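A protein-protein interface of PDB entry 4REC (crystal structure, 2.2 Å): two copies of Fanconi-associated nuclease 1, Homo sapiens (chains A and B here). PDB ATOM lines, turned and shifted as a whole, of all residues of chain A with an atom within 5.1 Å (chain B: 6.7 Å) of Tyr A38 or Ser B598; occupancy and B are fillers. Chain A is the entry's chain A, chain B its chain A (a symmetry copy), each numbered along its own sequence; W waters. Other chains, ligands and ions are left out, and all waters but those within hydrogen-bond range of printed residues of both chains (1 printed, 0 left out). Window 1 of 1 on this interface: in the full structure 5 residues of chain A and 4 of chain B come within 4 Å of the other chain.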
ATOM      1  N   LEU A  10      -3.001  -2.246  22.728  1.00  0.00           N
ATOM      2  CA  LEU A  10      -3.570  -1.120  21.974  1.00  0.00           C
ATOM      3  C   LEU A  10      -3.009  -1.036  20.537  1.00  0.00           C
ATOM      4  O   LEU A  10      -3.727  -0.695  19.595  1.00  0.00           O
ATOM      5  CB  LEU A  10      -3.338   0.176  22.732  1.00  0.00           C
ATOM      6  CG  LEU A  10      -4.220   0.264  23.982  1.00  0.00           C
ATOM      7  CD1 LEU A  10      -4.018   1.579  24.754  1.00  0.00           C
ATOM      8  CD2 LEU A  10      -5.670   0.120  23.580  1.00  0.00           C
ATOM      9  N   LEU A  13      -4.895  -3.624  18.282  1.00  0.00           N
ATOM     10  CA  LEU A  13      -6.252  -3.184  17.911  1.00  0.00           C
ATOM     11  C   LEU A  13      -6.228  -2.103  16.833  1.00  0.00           C
ATOM     12  O   LEU A  13      -7.055  -2.104  15.908  1.00  0.00           O
ATOM     13  CB  LEU A  13      -7.022  -2.634  19.112  1.00  0.00           C
ATOM     14  CG  LEU A  13      -7.584  -3.568  20.173  1.00  0.00           C
ATOM     15  CD1 LEU A  13      -8.474  -2.755  21.107  1.00  0.00           C
ATOM     16  CD2 LEU A  13      -8.351  -4.720  19.531  1.00  0.00           C
ATOM     17  N   LYS A  14      -5.301  -1.158  16.989  1.00  0.00           N
ATOM     18  CA  LYS A  14      -5.211  -0.026  16.076  1.00  0.00           C
ATOM     19  C   LYS A  14      -4.937  -0.537  14.668  1.00  0.00           C
ATOM     20  O   LYS A  14      -5.677  -0.243  13.730  1.00  0.00           O
ATOM     21  CB  LYS A  14      -4.110   0.949  16.519  1.00  0.00           C
ATOM     22  CG  LYS A  14      -4.109   2.272  15.762  1.00  0.00           C
ATOM     23  CD  LYS A  14      -2.798   3.051  15.948  1.00  0.00           C
ATOM     24  CE  LYS A  14      -2.472   3.322  17.428  1.00  0.00           C
ATOM     25  NZ  LYS A  14      -1.156   4.022  17.630  1.00  0.00           N
ATOM     26  N   LEU A  17      -7.964  -2.667  13.208  1.00  0.00           N
ATOM     27  CA  LEU A  17      -9.090  -1.761  12.970  1.00  0.00           C
ATOM     28  C   LEU A  17      -8.838  -0.856  11.768  1.00  0.00           C
ATOM     29  O   LEU A  17      -9.776  -0.477  11.072  1.00  0.00           O
ATOM     30  CB  LEU A  17      -9.368  -0.901  14.208  1.00  0.00           C
ATOM     31  CG  LEU A  17     -10.401  -1.287  15.284  1.00  0.00           C
ATOM     32  CD1 LEU A  17     -11.761  -0.686  14.975  1.00  0.00           C
ATOM     33  CD2 LEU A  17     -10.525  -2.795  15.441  1.00  0.00           C
ATOM     34  N   VAL A  34     -15.443  -4.026  20.505  1.00  0.00           N
ATOM     35  CA  VAL A  34     -14.191  -3.295  20.517  1.00  0.00           C
ATOM     36  C   VAL A  34     -14.475  -1.874  20.998  1.00  0.00           C
ATOM     37  O   VAL A  34     -13.740  -1.316  21.828  1.00  0.00           O
ATOM     38  CB  VAL A  34     -13.533  -3.278  19.138  1.00  0.00           C
ATOM     39  CG1 VAL A  34     -12.335  -2.316  19.123  1.00  0.00           C
ATOM     40  CG2 VAL A  34     -13.120  -4.691  18.725  1.00  0.00           C
ATOM     41  N   THR A  35     -15.561  -1.299  20.498  1.00  0.00           N
ATOM     42  CA  THR A  35     -15.986   0.008  20.971  1.00  0.00           C
ATOM     43  C   THR A  35     -16.165  -0.006  22.476  1.00  0.00           C
ATOM     44  O   THR A  35     -15.652   0.890  23.152  1.00  0.00           O
ATOM     45  CB  THR A  35     -17.279   0.452  20.315  1.00  0.00           C
ATOM     46  OG1 THR A  35     -17.055   0.606  18.908  1.00  0.00           O
ATOM     47  CG2 THR A  35     -17.744   1.775  20.903  1.00  0.00           C
ATOM     48  N   LYS A  36     -16.847  -1.040  23.007  1.00  0.00           N
ATOM     49  CA  LYS A  36     -17.096  -1.095  24.445  1.00  0.00           C
ATOM     50  C   LYS A  36     -15.800  -1.175  25.225  1.00  0.00           C
ATOM     51  O   LYS A  36     -15.690  -0.620  26.314  1.00  0.00           O
ATOM     52  CB  LYS A  36     -17.976  -2.279  24.820  1.00  0.00           C
ATOM     53  CG  LYS A  36     -19.452  -2.045  24.630  1.00  0.00           C
ATOM     54  CD  LYS A  36     -20.265  -2.894  25.598  1.00  0.00           C
ATOM     55  CE  LYS A  36     -20.208  -4.362  25.228  1.00  0.00           C
ATOM     56  NZ  LYS A  36     -20.742  -4.584  23.858  1.00  0.00           N
ATOM     57  N   PHE A  37     -14.817  -1.867  24.667  1.00  0.00           N
ATOM     58  CA  PHE A  37     -13.515  -1.970  25.323  1.00  0.00           C
ATOM     59  C   PHE A  37     -12.912  -0.580  25.415  1.00  0.00           C
ATOM     60  O   PHE A  37     -12.384  -0.184  26.464  1.00  0.00           O
ATOM     61  CB  PHE A  37     -12.567  -2.912  24.578  1.00  0.00           C
ATOM     62  CG  PHE A  37     -11.130  -2.852  25.071  1.00  0.00           C
ATOM     63  CD1 PHE A  37     -10.717  -3.606  26.155  1.00  0.00           C
ATOM     64  CD2 PHE A  37     -10.185  -2.040  24.427  1.00  0.00           C
ATOM     65  CE1 PHE A  37      -9.399  -3.552  26.606  1.00  0.00           C
ATOM     66  CE2 PHE A  37      -8.851  -1.959  24.871  1.00  0.00           C
ATOM     67  CZ  PHE A  37      -8.444  -2.705  25.954  1.00  0.00           C
ATOM     68  N   TYR A  38     -12.998   0.160  24.308  1.00  0.00           N
ATOM     69  CA  TYR A  38     -12.436   1.506  24.253  1.00  0.00           C
ATOM     70  C   TYR A  38     -13.149   2.428  25.256  1.00  0.00           C
ATOM     71  O   TYR A  38     -12.545   3.339  25.820  1.00  0.00           O
ATOM     72  CB  TYR A  38     -12.523   2.065  22.824  1.00  0.00           C
ATOM     73  CG  TYR A  38     -11.373   1.646  21.915  1.00  0.00           C
ATOM     74  CD1 TYR A  38     -10.064   1.594  22.392  1.00  0.00           C
ATOM     75  CD2 TYR A  38     -11.603   1.319  20.588  1.00  0.00           C
ATOM     76  CE1 TYR A  38      -9.006   1.228  21.560  1.00  0.00           C
ATOM     77  CE2 TYR A  38     -10.562   0.954  19.745  1.00  0.00           C
ATOM     78  CZ  TYR A  38      -9.271   0.910  20.230  1.00  0.00           C
ATOM     79  OH  TYR A  38      -8.256   0.549  19.378  1.00  0.00           O
ATOM     80  N   GLN A  39     -14.424   2.168  25.506  1.00  0.00           N
ATOM     81  CA  GLN A  39     -15.161   2.975  26.475  1.00  0.00           C
ATOM     82  C   GLN A  39     -14.888   2.624  27.934  1.00  0.00           C
ATOM     83  O   GLN A  39     -15.427   3.258  28.829  1.00  0.00           O
ATOM     84  CB  GLN A  39     -16.648   2.874  26.200  1.00  0.00           C
ATOM     85  CG  GLN A  39     -17.051   3.714  25.003  1.00  0.00           C
ATOM     86  CD  GLN A  39     -18.355   3.259  24.403  1.00  0.00           C
ATOM     87  OE1 GLN A  39     -18.925   2.248  24.827  1.00  0.00           O
ATOM     88  NE2 GLN A  39     -18.839   3.993  23.410  1.00  0.00           N
ATOM     89  N   LEU A  40     -14.049   1.628  28.185  1.00  0.00           N
ATOM     90  CA  LEU A  40     -13.734   1.273  29.558  1.00  0.00           C
ATOM     91  C   LEU A  40     -12.813   2.308  30.155  1.00  0.00           C
ATOM     92  O   LEU A  40     -11.984   2.880  29.457  1.00  0.00           O
ATOM     93  CB  LEU A  40     -13.047  -0.087  29.647  1.00  0.00           C
ATOM     94  CG  LEU A  40     -13.827  -1.364  29.361  1.00  0.00           C
ATOM     95  CD1 LEU A  40     -12.844  -2.498  29.151  1.00  0.00           C
ATOM     96  CD2 LEU A  40     -14.770  -1.667  30.514  1.00  0.00           C
ATOM     97  N   GLN A  45      -9.328  -1.168  31.488  1.00  0.00           N
ATOM     98  CA  GLN A  45      -8.665  -1.715  30.315  1.00  0.00           C
ATOM     99  C   GLN A  45      -7.478  -2.547  30.759  1.00  0.00           C
ATOM    100  O   GLN A  45      -7.220  -3.596  30.186  1.00  0.00           O
ATOM    101  CB  GLN A  45      -8.249  -0.604  29.343  1.00  0.00           C
ATOM    102  CG  GLN A  45      -9.447   0.044  28.646  1.00  0.00           C
ATOM    103  CD  GLN A  45      -9.051   1.105  27.623  1.00  0.00           C
ATOM    104  OE1 GLN A  45      -7.890   1.203  27.235  1.00  0.00           O
ATOM    105  NE2 GLN A  45     -10.024   1.884  27.168  1.00  0.00           N
ATOM    106  N   GLY B 456      -7.110   8.576  10.835  1.00  0.00           N
ATOM    107  CA  GLY B 456      -8.094   8.061  11.765  1.00  0.00           C
ATOM    108  C   GLY B 456      -8.495   8.996  12.897  1.00  0.00           C
ATOM    109  O   GLY B 456      -9.207   8.576  13.818  1.00  0.00           O
ATOM    110  N   PHE B 457      -8.057  10.254  12.853  1.00  0.00           N
ATOM    111  CA  PHE B 457      -8.471  11.184  13.890  1.00  0.00           C
ATOM    112  C   PHE B 457      -9.575  12.055  13.352  1.00  0.00           C
ATOM    113  O   PHE B 457      -9.327  13.134  12.800  1.00  0.00           O
ATOM    114  CB  PHE B 457      -7.293  12.012  14.388  1.00  0.00           C
ATOM    115  CG  PHE B 457      -6.163  11.174  14.950  1.00  0.00           C
ATOM    116  CD1 PHE B 457      -6.073  10.924  16.310  1.00  0.00           C
ATOM    117  CD2 PHE B 457      -5.209  10.645  14.120  1.00  0.00           C
ATOM    118  CE1 PHE B 457      -5.044  10.159  16.821  1.00  0.00           C
ATOM    119  CE2 PHE B 457      -4.180   9.883  14.622  1.00  0.00           C
ATOM    120  CZ  PHE B 457      -4.095   9.633  15.974  1.00  0.00           C
ATOM    121  N   CYS B 564     -11.290  12.178  26.472  1.00  0.00           N
ATOM    122  CA  CYS B 564     -10.098  11.603  25.840  1.00  0.00           C
ATOM    123  C   CYS B 564      -8.834  12.033  26.581  1.00  0.00           C
ATOM    124  O   CYS B 564      -7.921  11.248  26.750  1.00  0.00           O
ATOM    125  CB  CYS B 564     -10.002  12.007  24.363  1.00  0.00           C
ATOM    126  SG  CYS B 564     -11.420  11.510  23.355  1.00  0.00           S
ATOM    127  N   TRP B 594      -8.424  14.058  17.739  1.00  0.00           N
ATOM    128  CA  TRP B 594      -8.738  12.781  18.354  1.00  0.00           C
ATOM    129  C   TRP B 594      -9.689  11.879  17.577  1.00  0.00           C
ATOM    130  O   TRP B 594     -10.512  12.324  16.743  1.00  0.00           O
ATOM    131  CB  TRP B 594      -9.274  13.006  19.771  1.00  0.00           C
ATOM    132  CG  TRP B 594     -10.626  13.551  19.883  1.00  0.00           C
ATOM    133  CD1 TRP B 594     -11.782  12.839  20.100  1.00  0.00           C
ATOM    134  CD2 TRP B 594     -11.012  14.933  19.846  1.00  0.00           C
ATOM    135  NE1 TRP B 594     -12.856  13.689  20.192  1.00  0.00           N
ATOM    136  CE2 TRP B 594     -12.421  14.979  20.045  1.00  0.00           C
ATOM    137  CE3 TRP B 594     -10.315  16.135  19.664  1.00  0.00           C
ATOM    138  CZ2 TRP B 594     -13.139  16.180  20.062  1.00  0.00           C
ATOM    139  CZ3 TRP B 594     -11.026  17.327  19.664  1.00  0.00           C
ATOM    140  CH2 TRP B 594     -12.423  17.346  19.866  1.00  0.00           C
ATOM    141  N   ASN B 595      -9.486  10.591  17.859  1.00  0.00           N
ATOM    142  CA  ASN B 595     -10.271   9.478  17.360  1.00  0.00           C
ATOM    143  C   ASN B 595     -11.433   9.245  18.307  1.00  0.00           C
ATOM    144  O   ASN B 595     -11.209   8.857  19.443  1.00  0.00           O
ATOM    145  CB  ASN B 595      -9.385   8.225  17.269  1.00  0.00           C
ATOM    146  CG  ASN B 595     -10.113   7.022  16.715  1.00  0.00           C
ATOM    147  OD1 ASN B 595     -11.271   6.745  17.075  1.00  0.00           O
ATOM    148  ND2 ASN B 595      -9.436   6.290  15.827  1.00  0.00           N
ATOM    149  N   SER B 596     -12.661   9.469  17.861  1.00  0.00           N
ATOM    150  CA  SER B 596     -13.790   9.399  18.789  1.00  0.00           C
ATOM    151  C   SER B 596     -14.121   7.962  19.239  1.00  0.00           C
ATOM    152  O   SER B 596     -14.844   7.792  20.204  1.00  0.00           O
ATOM    153  CB  SER B 596     -15.038  10.036  18.177  1.00  0.00           C
ATOM    154  OG  SER B 596     -15.261   9.533  16.874  1.00  0.00           O
ATOM    155  N   GLN B 597     -13.603   6.945  18.550  1.00  0.00           N
ATOM    156  CA  GLN B 597     -13.864   5.569  18.962  1.00  0.00           C
ATOM    157  C   GLN B 597     -12.849   5.102  19.996  1.00  0.00           C
ATOM    158  O   GLN B 597     -13.216   4.705  21.095  1.00  0.00           O
ATOM    159  CB  GLN B 597     -13.855   4.606  17.775  1.00  0.00           C
ATOM    160  CG  GLN B 597     -14.364   3.229  18.183  1.00  0.00           C
ATOM    161  CD  GLN B 597     -14.062   2.132  17.172  1.00  0.00           C
ATOM    162  OE1 GLN B 597     -13.284   2.323  16.227  1.00  0.00           O
ATOM    163  NE2 GLN B 597     -14.673   0.964  17.377  1.00  0.00           N
ATOM    164  N   SER B 598     -11.570   5.156  19.650  1.00  0.00           N
ATOM    165  CA  SER B 598     -10.544   4.682  20.562  1.00  0.00           C
ATOM    166  C   SER B 598     -10.181   5.699  21.634  1.00  0.00           C
ATOM    167  O   SER B 598      -9.480   5.360  22.591  1.00  0.00           O
ATOM    168  CB  SER B 598      -9.288   4.320  19.782  1.00  0.00           C
ATOM    169  OG  SER B 598      -8.748   5.493  19.185  1.00  0.00           O
ATOM    170  N   ARG B 599     -10.597   6.951  21.437  1.00  0.00           N
ATOM    171  CA  ARG B 599     -10.223   8.057  22.327  1.00  0.00           C
ATOM    172  C   ARG B 599      -8.718   8.337  22.355  1.00  0.00           C
ATOM    173  O   ARG B 599      -8.193   8.964  23.287  1.00  0.00           O
ATOM    174  CB  ARG B 599     -10.722   7.787  23.745  1.00  0.00           C
ATOM    175  CG  ARG B 599     -12.206   7.549  23.767  1.00  0.00           C
ATOM    176  CD  ARG B 599     -12.742   7.274  25.138  1.00  0.00           C
ATOM    177  NE  ARG B 599     -14.192   7.371  25.105  1.00  0.00           N
ATOM    178  CZ  ARG B 599     -14.967   7.217  26.167  1.00  0.00           C
ATOM    179  NH1 ARG B 599     -14.419   6.946  27.346  1.00  0.00           N
ATOM    180  NH2 ARG B 599     -16.284   7.333  26.047  1.00  0.00           N
ATOM    181  N   HIS B 600      -8.026   7.846  21.342  1.00  0.00           N
ATOM    182  CA  HIS B 600      -6.652   8.249  21.099  1.00  0.00           C
ATOM    183  C   HIS B 600      -6.616   9.736  20.687  1.00  0.00           C
ATOM    184  O   HIS B 600      -7.364  10.180  19.787  1.00  0.00           O
ATOM    185  CB  HIS B 600      -6.033   7.369  20.012  1.00  0.00           C
ATOM    186  CG  HIS B 600      -4.554   7.539  19.855  1.00  0.00           C
ATOM    187  ND1 HIS B 600      -3.876   7.102  18.739  1.00  0.00           N
ATOM    188  CD2 HIS B 600      -3.627   8.079  20.679  1.00  0.00           C
ATOM    189  CE1 HIS B 600      -2.589   7.359  18.885  1.00  0.00           C
ATOM    190  NE2 HIS B 600      -2.411   7.954  20.048  1.00  0.00           N
ATOM    191  N   PHE B 601      -5.780  10.511  21.367  1.00  0.00           N
ATOM    192  CA  PHE B 601      -5.607  11.913  21.009  1.00  0.00           C
ATOM    193  C   PHE B 601      -4.119  12.217  20.829  1.00  0.00           C
ATOM    194  O   PHE B 601      -3.250  11.526  21.405  1.00  0.00           O
ATOM    195  CB  PHE B 601      -6.213  12.847  22.061  1.00  0.00           C
ATOM    196  CG  PHE B 601      -5.419  12.919  23.331  1.00  0.00           C
ATOM    197  CD1 PHE B 601      -5.638  11.985  24.354  1.00  0.00           C
ATOM    198  CD2 PHE B 601      -4.420  13.888  23.499  1.00  0.00           C
ATOM    199  CE1 PHE B 601      -4.892  12.038  25.533  1.00  0.00           C
ATOM    200  CE2 PHE B 601      -3.659  13.953  24.662  1.00  0.00           C
ATOM    201  CZ  PHE B 601      -3.892  13.040  25.690  1.00  0.00           C
HETATM  202  O   HOH W   1      -9.809   4.096  25.184  1.00  0.00           O
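The side-chain amide nitrogen (NE2) of Gln B597 is in hydrogen-bond range of the side-chain hydroxyl (OG1) of Thr A35 (2.9 Å).
O of Tyr A38 is in hydrogen-bond range of NE2 of Gln A45 (3.2 Å).
OD1 of Asn B595 sits at hydrogen-bond distance from N of Gln B597, at 2.8 Å.
The backbone NH of Ser B598 sits at hydrogen-bond distance from the side-chain amide oxygen of Asn B595 (3.0 Å).
The backbone NH of Asn B595 lies within hydrogen-bond range of the backbone carbonyl oxygen of His B600.
OG of Ser B598 sits close to N of His B600 (3.3 Å).
Among the printed residues, merely in contact across the chains: Tyr A38 with Gln B597 (3.2 Å), Tyr A38 with Ser B598 (3.4 Å), Leu A17 with Gln B597 (3.6 Å), Lys A14 with His B600 (3.8 Å), Gln A39 with Arg B599 (3.8 Å) and Tyr A38 with Arg B599 (3.999 Å).
Printed residues of chain B within 4 Å of Tyr A38: Gln B597 (3.2 Å), Ser B598 (3.4 Å) and Arg B599 (3.999 Å).
Ser B598 touches just one residue of chain A: Tyr A38.
Printed residues of chain A within 4 Å of Gln B597: Leu A17 (3.6 Å), Thr A35 (2.9 Å) and Tyr A38 (3.2 Å).
Of the printed residues of chain A, Arg B599 touches Tyr A38 and Gln A39.
Of the printed residues of chain B, Gln A39 touches Arg B599 (3.8 Å).
The nearest printed residue of chain A that does not touch Ser B598 is Gln A45 (5.8 Å).
The nearest printed residue of chain B that does not touch Gln A39 is Gln B597 (5.2 Å).
Of the 12 printed residues of chain A, 5 touch a printed residue of chain B.
Among the printed residues, 7 pairs touch across the chains.
Among the printed residues, no Asp or Glu carboxylate lies within 4 Å of a Lys or Arg side-chain nitrogen of the other chain.
No position is printed for both chains.
Of the 7 pairs that touch across the chains among the printed residues, none has its exchanged pair printed and touching as well.
Water W1 lies within hydrogen-bond range of O of Ser B598 (2.9 Å), O of Tyr A38 (2.9 Å) and NE2 of Gln A45 (3.0 Å).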
